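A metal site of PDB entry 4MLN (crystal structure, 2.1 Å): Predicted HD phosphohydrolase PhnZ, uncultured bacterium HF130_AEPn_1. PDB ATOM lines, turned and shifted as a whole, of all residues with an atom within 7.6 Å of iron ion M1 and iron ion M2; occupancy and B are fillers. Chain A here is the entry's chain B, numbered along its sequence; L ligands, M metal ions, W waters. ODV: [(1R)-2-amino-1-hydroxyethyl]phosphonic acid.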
ATOM      1  N   TYR A  24       4.276  -0.089  35.951  1.00  0.00           N
ATOM      2  CA  TYR A  24       4.554   0.525  34.639  1.00  0.00           C
ATOM      3  C   TYR A  24       4.344   2.026  34.791  1.00  0.00           C
ATOM      4  O   TYR A  24       5.227   2.841  34.495  1.00  0.00           O
ATOM      5  CB  TYR A  24       3.604  -0.038  33.574  1.00  0.00           C
ATOM      6  CG  TYR A  24       3.948   0.279  32.112  1.00  0.00           C
ATOM      7  CD1 TYR A  24       4.910  -0.463  31.419  1.00  0.00           C
ATOM      8  CD2 TYR A  24       3.277   1.294  31.426  1.00  0.00           C
ATOM      9  CE1 TYR A  24       5.226  -0.176  30.086  1.00  0.00           C
ATOM     10  CE2 TYR A  24       3.585   1.580  30.087  1.00  0.00           C
ATOM     11  CZ  TYR A  24       4.554   0.840  29.417  1.00  0.00           C
ATOM     12  OH  TYR A  24       4.850   1.117  28.078  1.00  0.00           O
ATOM     13  N   GLN A  31       1.965  -3.347  34.915  1.00  0.00           N
ATOM     14  CA  GLN A  31       2.344  -3.853  33.597  1.00  0.00           C
ATOM     15  C   GLN A  31       1.225  -4.627  32.910  1.00  0.00           C
ATOM     16  O   GLN A  31       1.032  -4.521  31.688  1.00  0.00           O
ATOM     17  CB  GLN A  31       3.626  -4.696  33.680  1.00  0.00           C
ATOM     18  N   HIS A  34      -1.543  -2.347  31.694  1.00  0.00           N
ATOM     19  CA  HIS A  34      -1.007  -1.735  30.481  1.00  0.00           C
ATOM     20  C   HIS A  34      -1.242  -2.640  29.272  1.00  0.00           C
ATOM     21  O   HIS A  34      -1.948  -2.269  28.336  1.00  0.00           O
ATOM     22  CB  HIS A  34       0.502  -1.457  30.643  1.00  0.00           C
ATOM     23  CG  HIS A  34       1.123  -0.860  29.423  1.00  0.00           C
ATOM     24  ND1 HIS A  34       0.657   0.295  28.829  1.00  0.00           N
ATOM     25  CD2 HIS A  34       2.195  -1.258  28.687  1.00  0.00           C
ATOM     26  CE1 HIS A  34       1.397   0.580  27.777  1.00  0.00           C
ATOM     27  NE2 HIS A  34       2.344  -0.347  27.671  1.00  0.00           N
ATOM     28  N   SER A  35      -0.660  -3.823  29.295  1.00  0.00           N
ATOM     29  CA  SER A  35      -0.762  -4.756  28.188  1.00  0.00           C
ATOM     30  C   SER A  35      -2.205  -5.005  27.800  1.00  0.00           C
ATOM     31  O   SER A  35      -2.557  -4.927  26.625  1.00  0.00           O
ATOM     32  CB  SER A  35      -0.093  -6.063  28.548  1.00  0.00           C
ATOM     33  OG  SER A  35       1.255  -5.853  28.904  1.00  0.00           O
ATOM     34  N   CYS A  38      -3.855  -2.081  25.837  1.00  0.00           N
ATOM     35  CA  CYS A  38      -3.418  -2.022  24.463  1.00  0.00           C
ATOM     36  C   CYS A  38      -4.141  -3.084  23.614  1.00  0.00           C
ATOM     37  O   CYS A  38      -4.719  -2.758  22.576  1.00  0.00           O
ATOM     38  CB  CYS A  38      -1.898  -2.186  24.391  1.00  0.00           C
ATOM     39  SG  CYS A  38      -0.969  -0.840  25.241  1.00  0.00           S
ATOM     40  N   ALA A  55       0.089  -5.827  20.135  1.00  0.00           N
ATOM     41  CA  ALA A  55      -0.348  -4.873  21.151  1.00  0.00           C
ATOM     42  C   ALA A  55      -0.300  -5.483  22.572  1.00  0.00           C
ATOM     43  O   ALA A  55       0.272  -4.905  23.507  1.00  0.00           O
ATOM     44  CB  ALA A  55      -1.759  -4.378  20.838  1.00  0.00           C
ATOM     45  N   HIS A  58       3.710  -6.280  23.484  1.00  0.00           N
ATOM     46  CA  HIS A  58       4.808  -5.406  23.044  1.00  0.00           C
ATOM     47  C   HIS A  58       5.836  -5.151  24.146  1.00  0.00           C
ATOM     48  O   HIS A  58       7.000  -4.916  23.855  1.00  0.00           O
ATOM     49  CB  HIS A  58       4.269  -4.071  22.508  1.00  0.00           C
ATOM     50  CG  HIS A  58       3.805  -3.138  23.582  1.00  0.00           C
ATOM     51  ND1 HIS A  58       2.547  -3.210  24.130  1.00  0.00           N
ATOM     52  CD2 HIS A  58       4.435  -2.123  24.216  1.00  0.00           C
ATOM     53  CE1 HIS A  58       2.417  -2.265  25.051  1.00  0.00           C
ATOM     54  NE2 HIS A  58       3.551  -1.596  25.120  1.00  0.00           N
ATOM     55  N   ASP A  59       5.384  -5.194  25.403  1.00  0.00           N
ATOM     56  CA  ASP A  59       6.266  -4.973  26.553  1.00  0.00           C
ATOM     57  C   ASP A  59       6.680  -6.241  27.281  1.00  0.00           C
ATOM     58  O   ASP A  59       7.193  -6.183  28.391  1.00  0.00           O
ATOM     59  CB  ASP A  59       5.645  -3.973  27.528  1.00  0.00           C
ATOM     60  CG  ASP A  59       5.892  -2.536  27.127  1.00  0.00           C
ATOM     61  OD1 ASP A  59       6.880  -2.269  26.425  1.00  0.00           O
ATOM     62  OD2 ASP A  59       5.107  -1.668  27.524  1.00  0.00           O
ATOM     63  N   LEU A  60       6.493  -7.386  26.643  1.00  0.00           N
ATOM     64  CA  LEU A  60       6.860  -8.667  27.219  1.00  0.00           C
ATOM     65  C   LEU A  60       8.289  -8.668  27.745  1.00  0.00           C
ATOM     66  O   LEU A  60       8.590  -9.245  28.799  1.00  0.00           O
ATOM     67  CB  LEU A  60       6.708  -9.761  26.173  1.00  0.00           C
ATOM     68  CG  LEU A  60       6.904 -11.215  26.638  1.00  0.00           C
ATOM     69  CD1 LEU A  60       5.863 -11.612  27.695  1.00  0.00           C
ATOM     70  CD2 LEU A  60       6.832 -12.129  25.438  1.00  0.00           C
ATOM     71  N   HIS A  62       9.968  -6.654  29.225  1.00  0.00           N
ATOM     72  CA  HIS A  62      10.157  -6.105  30.562  1.00  0.00           C
ATOM     73  C   HIS A  62      10.100  -7.183  31.641  1.00  0.00           C
ATOM     74  O   HIS A  62      10.527  -6.952  32.763  1.00  0.00           O
ATOM     75  CB  HIS A  62       9.115  -5.047  30.886  1.00  0.00           C
ATOM     76  CG  HIS A  62       9.361  -3.723  30.238  1.00  0.00           C
ATOM     77  ND1 HIS A  62      10.624  -3.205  30.052  1.00  0.00           N
ATOM     78  CD2 HIS A  62       8.494  -2.802  29.764  1.00  0.00           C
ATOM     79  CE1 HIS A  62      10.525  -2.018  29.473  1.00  0.00           C
ATOM     80  NE2 HIS A  62       9.246  -1.750  29.288  1.00  0.00           N
ATOM     81  N   HIS A  80      14.129  -4.008  25.788  1.00  0.00           N
ATOM     82  CA  HIS A  80      12.960  -4.819  26.087  1.00  0.00           C
ATOM     83  C   HIS A  80      12.211  -5.173  24.802  1.00  0.00           C
ATOM     84  O   HIS A  80      11.630  -6.251  24.703  1.00  0.00           O
ATOM     85  CB  HIS A  80      12.028  -4.131  27.105  1.00  0.00           C
ATOM     86  CG  HIS A  80      11.264  -2.956  26.541  1.00  0.00           C
ATOM     87  ND1 HIS A  80      11.867  -1.765  26.216  1.00  0.00           N
ATOM     88  CD2 HIS A  80       9.936  -2.786  26.314  1.00  0.00           C
ATOM     89  CE1 HIS A  80      10.949  -0.913  25.779  1.00  0.00           C
ATOM     90  NE2 HIS A  80       9.770  -1.514  25.847  1.00  0.00           N
ATOM     91  N   GLU A  81      12.226  -4.265  23.826  1.00  0.00           N
ATOM     92  CA  GLU A  81      11.546  -4.535  22.561  1.00  0.00           C
ATOM     93  C   GLU A  81      12.143  -5.747  21.845  1.00  0.00           C
ATOM     94  O   GLU A  81      11.428  -6.602  21.323  1.00  0.00           O
ATOM     95  CB  GLU A  81      11.494  -3.287  21.656  1.00  0.00           C
ATOM     96  CG  GLU A  81      12.798  -2.927  20.950  1.00  0.00           C
ATOM     97  CD  GLU A  81      13.827  -2.229  21.841  1.00  0.00           C
ATOM     98  OE1 GLU A  81      13.699  -2.178  23.083  1.00  0.00           O
ATOM     99  OE2 GLU A  81      14.814  -1.714  21.282  1.00  0.00           O
ATOM    100  N   ILE A 101       6.596  -5.689  17.447  1.00  0.00           N
ATOM    101  CA  ILE A 101       6.998  -5.491  18.826  1.00  0.00           C
ATOM    102  C   ILE A 101       8.354  -4.803  18.852  1.00  0.00           C
ATOM    103  O   ILE A 101       8.560  -3.815  19.560  1.00  0.00           O
ATOM    104  CB  ILE A 101       7.045  -6.813  19.609  1.00  0.00           C
ATOM    105  CG1 ILE A 101       5.622  -7.302  19.861  1.00  0.00           C
ATOM    106  CG2 ILE A 101       7.734  -6.608  20.949  1.00  0.00           C
ATOM    107  CD1 ILE A 101       5.541  -8.716  20.390  1.00  0.00           C
ATOM    108  N   HIS A 104       8.196  -1.005  18.159  1.00  0.00           N
ATOM    109  CA  HIS A 104       7.481  -0.060  19.006  1.00  0.00           C
ATOM    110  C   HIS A 104       8.381   0.972  19.669  1.00  0.00           C
ATOM    111  O   HIS A 104       7.925   2.062  20.007  1.00  0.00           O
ATOM    112  CB  HIS A 104       6.559  -0.771  20.034  1.00  0.00           C
ATOM    113  CG  HIS A 104       7.177  -1.029  21.381  1.00  0.00           C
ATOM    114  ND1 HIS A 104       7.870  -2.188  21.667  1.00  0.00           N
ATOM    115  CD2 HIS A 104       7.125  -0.333  22.538  1.00  0.00           C
ATOM    116  CE1 HIS A 104       8.243  -2.169  22.936  1.00  0.00           C
ATOM    117  NE2 HIS A 104       7.802  -1.060  23.482  1.00  0.00           N
ATOM    118  N   VAL A 105       9.645   0.645  19.858  1.00  0.00           N
ATOM    119  CA  VAL A 105      10.579   1.621  20.393  1.00  0.00           C
ATOM    120  C   VAL A 105      11.094   2.540  19.266  1.00  0.00           C
ATOM    121  O   VAL A 105      11.279   3.749  19.459  1.00  0.00           O
ATOM    122  CB  VAL A 105      11.733   0.934  21.142  1.00  0.00           C
ATOM    123  CG1 VAL A 105      12.919   1.899  21.389  1.00  0.00           C
ATOM    124  CG2 VAL A 105      11.214   0.369  22.469  1.00  0.00           C
ATOM    125  N   LYS A 108       8.609   5.199  18.720  1.00  0.00           N
ATOM    126  CA  LYS A 108       8.783   6.309  19.649  1.00  0.00           C
ATOM    127  C   LYS A 108       9.895   7.255  19.187  1.00  0.00           C
ATOM    128  O   LYS A 108       9.715   8.470  19.118  1.00  0.00           O
ATOM    129  CB  LYS A 108       9.084   5.804  21.063  1.00  0.00           C
ATOM    130  CG  LYS A 108       9.475   6.916  22.043  1.00  0.00           C
ATOM    131  CD  LYS A 108       9.482   6.425  23.499  1.00  0.00           C
ATOM    132  CE  LYS A 108      10.596   5.455  23.769  1.00  0.00           C
ATOM    133  NZ  LYS A 108      10.768   5.242  25.230  1.00  0.00           N
ATOM    134  N   SER A 126       8.814   6.869  29.926  1.00  0.00           N
ATOM    135  CA  SER A 126       9.109   6.743  28.506  1.00  0.00           C
ATOM    136  C   SER A 126      10.051   7.808  27.980  1.00  0.00           C
ATOM    137  O   SER A 126      10.772   7.559  27.025  1.00  0.00           O
ATOM    138  CB  SER A 126       7.844   6.716  27.659  1.00  0.00           C
ATOM    139  OG  SER A 126       7.299   5.415  27.676  1.00  0.00           O
ATOM    140  N   THR A 129      13.497   6.386  29.218  1.00  0.00           N
ATOM    141  CA  THR A 129      13.942   5.180  28.529  1.00  0.00           C
ATOM    142  C   THR A 129      14.479   5.520  27.144  1.00  0.00           C
ATOM    143  O   THR A 129      15.325   4.821  26.587  1.00  0.00           O
ATOM    144  CB  THR A 129      12.827   4.097  28.456  1.00  0.00           C
ATOM    145  OG1 THR A 129      11.732   4.544  27.635  1.00  0.00           O
ATOM    146  CG2 THR A 129      12.320   3.776  29.846  1.00  0.00           C
ATOM    147  N   GLN A 133      17.805   4.357  24.556  1.00  0.00           N
ATOM    148  CA  GLN A 133      17.349   3.724  23.323  1.00  0.00           C
ATOM    149  C   GLN A 133      17.927   4.406  22.083  1.00  0.00           C
ATOM    150  O   GLN A 133      17.555   4.074  20.954  1.00  0.00           O
ATOM    151  CB  GLN A 133      15.814   3.703  23.268  1.00  0.00           C
ATOM    152  CG  GLN A 133      15.146   2.793  24.357  1.00  0.00           C
ATOM    153  CD  GLN A 133      13.654   3.104  24.599  1.00  0.00           C
ATOM    154  OE1 GLN A 133      13.169   4.210  24.309  1.00  0.00           O
ATOM    155  NE2 GLN A 133      12.932   2.129  25.163  1.00  0.00           N
ATOM    156  N   ILE A 157       0.705   0.721  16.826  1.00  0.00           N
ATOM    157  CA  ILE A 157       1.096   0.081  18.080  1.00  0.00           C
ATOM    158  C   ILE A 157       1.476   1.119  19.129  1.00  0.00           C
ATOM    159  O   ILE A 157       0.988   1.096  20.261  1.00  0.00           O
ATOM    160  CB  ILE A 157       2.252  -0.937  17.845  1.00  0.00           C
ATOM    161  CG1 ILE A 157       1.766  -2.067  16.926  1.00  0.00           C
ATOM    162  CG2 ILE A 157       2.800  -1.489  19.170  1.00  0.00           C
ATOM    163  CD1 ILE A 157       0.651  -2.917  17.514  1.00  0.00           C
ATOM    164  N   ARG A 158       2.343   2.053  18.737  1.00  0.00           N
ATOM    165  CA  ARG A 158       2.832   3.056  19.689  1.00  0.00           C
ATOM    166  C   ARG A 158       1.722   3.988  20.170  1.00  0.00           C
ATOM    167  O   ARG A 158       1.717   4.425  21.326  1.00  0.00           O
ATOM    168  CB  ARG A 158       3.979   3.867  19.088  1.00  0.00           C
ATOM    169  CG  ARG A 158       4.672   4.688  20.127  1.00  0.00           C
ATOM    170  CD  ARG A 158       5.543   3.779  21.007  1.00  0.00           C
ATOM    171  NE  ARG A 158       5.737   4.354  22.312  1.00  0.00           N
ATOM    172  CZ  ARG A 158       6.651   3.939  23.175  1.00  0.00           C
ATOM    173  NH1 ARG A 158       7.459   2.944  22.852  1.00  0.00           N
ATOM    174  NH2 ARG A 158       6.742   4.539  24.358  1.00  0.00           N
ATOM    175  N   TRP A 160      -1.488   3.119  20.613  1.00  0.00           N
ATOM    176  CA  TRP A 160      -2.166   2.378  21.667  1.00  0.00           C
ATOM    177  C   TRP A 160      -1.316   2.316  22.941  1.00  0.00           C
ATOM    178  O   TRP A 160      -1.839   2.459  24.053  1.00  0.00           O
ATOM    179  CB  TRP A 160      -2.478   0.973  21.181  1.00  0.00           C
ATOM    180  CG  TRP A 160      -3.489   0.900  20.071  1.00  0.00           C
ATOM    181  CD1 TRP A 160      -4.565   1.724  19.878  1.00  0.00           C
ATOM    182  CD2 TRP A 160      -3.496  -0.037  18.992  1.00  0.00           C
ATOM    183  NE1 TRP A 160      -5.264   1.334  18.754  1.00  0.00           N
ATOM    184  CE2 TRP A 160      -4.626   0.263  18.192  1.00  0.00           C
ATOM    185  CE3 TRP A 160      -2.674  -1.106  18.624  1.00  0.00           C
ATOM    186  CZ2 TRP A 160      -4.936  -0.469  17.048  1.00  0.00           C
ATOM    187  CZ3 TRP A 160      -2.986  -1.836  17.497  1.00  0.00           C
ATOM    188  CH2 TRP A 160      -4.108  -1.513  16.713  1.00  0.00           C
ATOM    189  N   ASP A 161      -0.014   2.114  22.746  1.00  0.00           N
ATOM    190  CA  ASP A 161       0.985   2.103  23.814  1.00  0.00           C
ATOM    191  C   ASP A 161       0.836   3.350  24.689  1.00  0.00           C
ATOM    192  O   ASP A 161       0.676   3.250  25.900  1.00  0.00           O
ATOM    193  CB  ASP A 161       2.396   2.065  23.201  1.00  0.00           C
ATOM    194  CG  ASP A 161       3.493   1.662  24.205  1.00  0.00           C
ATOM    195  OD1 ASP A 161       3.203   1.498  25.420  1.00  0.00           O
ATOM    196  OD2 ASP A 161       4.665   1.528  23.779  1.00  0.00           O
ATOM    197  N   GLU A 162       0.859   4.510  24.060  1.00  0.00           N
ATOM    198  CA  GLU A 162       0.801   5.768  24.800  1.00  0.00           C
ATOM    199  C   GLU A 162      -0.550   5.957  25.474  1.00  0.00           C
ATOM    200  O   GLU A 162      -0.645   6.581  26.525  1.00  0.00           O
ATOM    201  CB  GLU A 162       1.129   6.952  23.870  1.00  0.00           C
ATOM    202  CG  GLU A 162       2.500   7.578  24.093  1.00  0.00           C
ATOM    203  CD  GLU A 162       3.659   6.645  23.748  1.00  0.00           C
ATOM    204  OE1 GLU A 162       4.102   5.890  24.636  1.00  0.00           O
ATOM    205  OE2 GLU A 162       4.132   6.662  22.587  1.00  0.00           O
ATOM    206  N   GLY A 164      -2.441   3.470  26.638  1.00  0.00           N
ATOM    207  CA  GLY A 164      -2.637   2.404  27.612  1.00  0.00           C
ATOM    208  C   GLY A 164      -2.245   2.728  29.050  1.00  0.00           C
ATOM    209  O   GLY A 164      -1.441   2.030  29.656  1.00  0.00           O
HETATM  210  OAD ODV L   1      10.528   2.444  26.462  1.00  0.00           O
HETATM  211  PAH ODV L   1       9.050   2.252  26.318  1.00  0.00           P
HETATM  212  OAE ODV L   1       8.887   1.382  25.122  1.00  0.00           O
HETATM  213  OAB ODV L   1       8.506   3.596  25.985  1.00  0.00           O
HETATM  214  CAG ODV L   1       8.176   1.531  27.749  1.00  0.00           C
HETATM  215  OAC ODV L   1       7.978   0.183  27.549  1.00  0.00           O
HETATM  216  CAF ODV L   1       8.945   1.770  28.991  1.00  0.00           C
HETATM  217  NAA ODV L   1       7.968   1.977  30.025  1.00  0.00           N
HETATM  218 FE    FE M   1       4.149  -0.171  26.522  1.00  0.00          FE
HETATM  219 FE    FE M   2       7.830  -0.526  25.577  1.00  0.00          FE
HETATM  220  O   HOH W   1       6.138   0.488  25.659  1.00  0.00           O
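An oxygen (OAC) of the ligand sits close to a ring nitrogen (NE2) of His 62 (2.9 Å). An oxygen (OAB) of the ligand lies within salt-bridge range of the guanidinium group of Arg 158 (2.6 Å). The side-chain amide nitrogen of Gln 133 lies within hydrogen-bond range of an oxygen (OAD) of the ligand, at 2.8 Å. OG of Ser 126 is in hydrogen-bond range of OAB of the ligand, 2.8 Å away. The side-chain amino group (NZ) of Lys 108 is in salt-bridge range of an oxygen (OAB) of the ligand, 2.9 Å away. An oxygen (OAD) of the ligand lies within hydrogen-bond range of the side-chain hydroxyl (OG1) of Thr 129 (2.7 Å).
ND1 of His 58 lies within hydrogen-bond range of O of Ala 55, 2.9 Å away. O of His 34 sits at hydrogen-bond distance from SG of Cys 38 (3.5 Å). The backbone carbonyl oxygen (O) of Gly 164 lies within hydrogen-bond range of a ring nitrogen (ND1) of His 34. The backbone carbonyl oxygen (O) of His 104 sits at hydrogen-bond distance from the guanidinium group (NH1) of Arg 158 (3.0 Å). A ring nitrogen (ND1) of His 104 lies within hydrogen-bond range of the backbone carbonyl oxygen of Ile 101 (2.8 Å). NE2 of His 80 sits close to NE2 of His 62 (3.5 Å). OD2 of Asp 161 lies within salt-bridge range of NH1 of Arg 158.
Iron ion M2 is bound by water W1, OAC of the ligand, OD1 of Asp 59, NE2 of His 104, NE2 of His 80 and OAE of the ligand. Iron ion M2 has six donor atoms within binding distance.
Of the 25 residues printed, 5 come within 4 Å of iron ion M1.
The nearest printed residue that does not touch iron ion M2 is His 62 (4.2 Å).
Iron ion M1 is bound by OD2 of Asp 59 (2.0 Å), NE2 of His 58 (2.1 Å), OH of Tyr 24 (2.1 Å), NE2 of His 34 (2.1 Å), OD1 of Asp 161 (2.2 Å) and water W1 (2.3 Å). Iron ion M1 has six donor atoms within binding distance.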
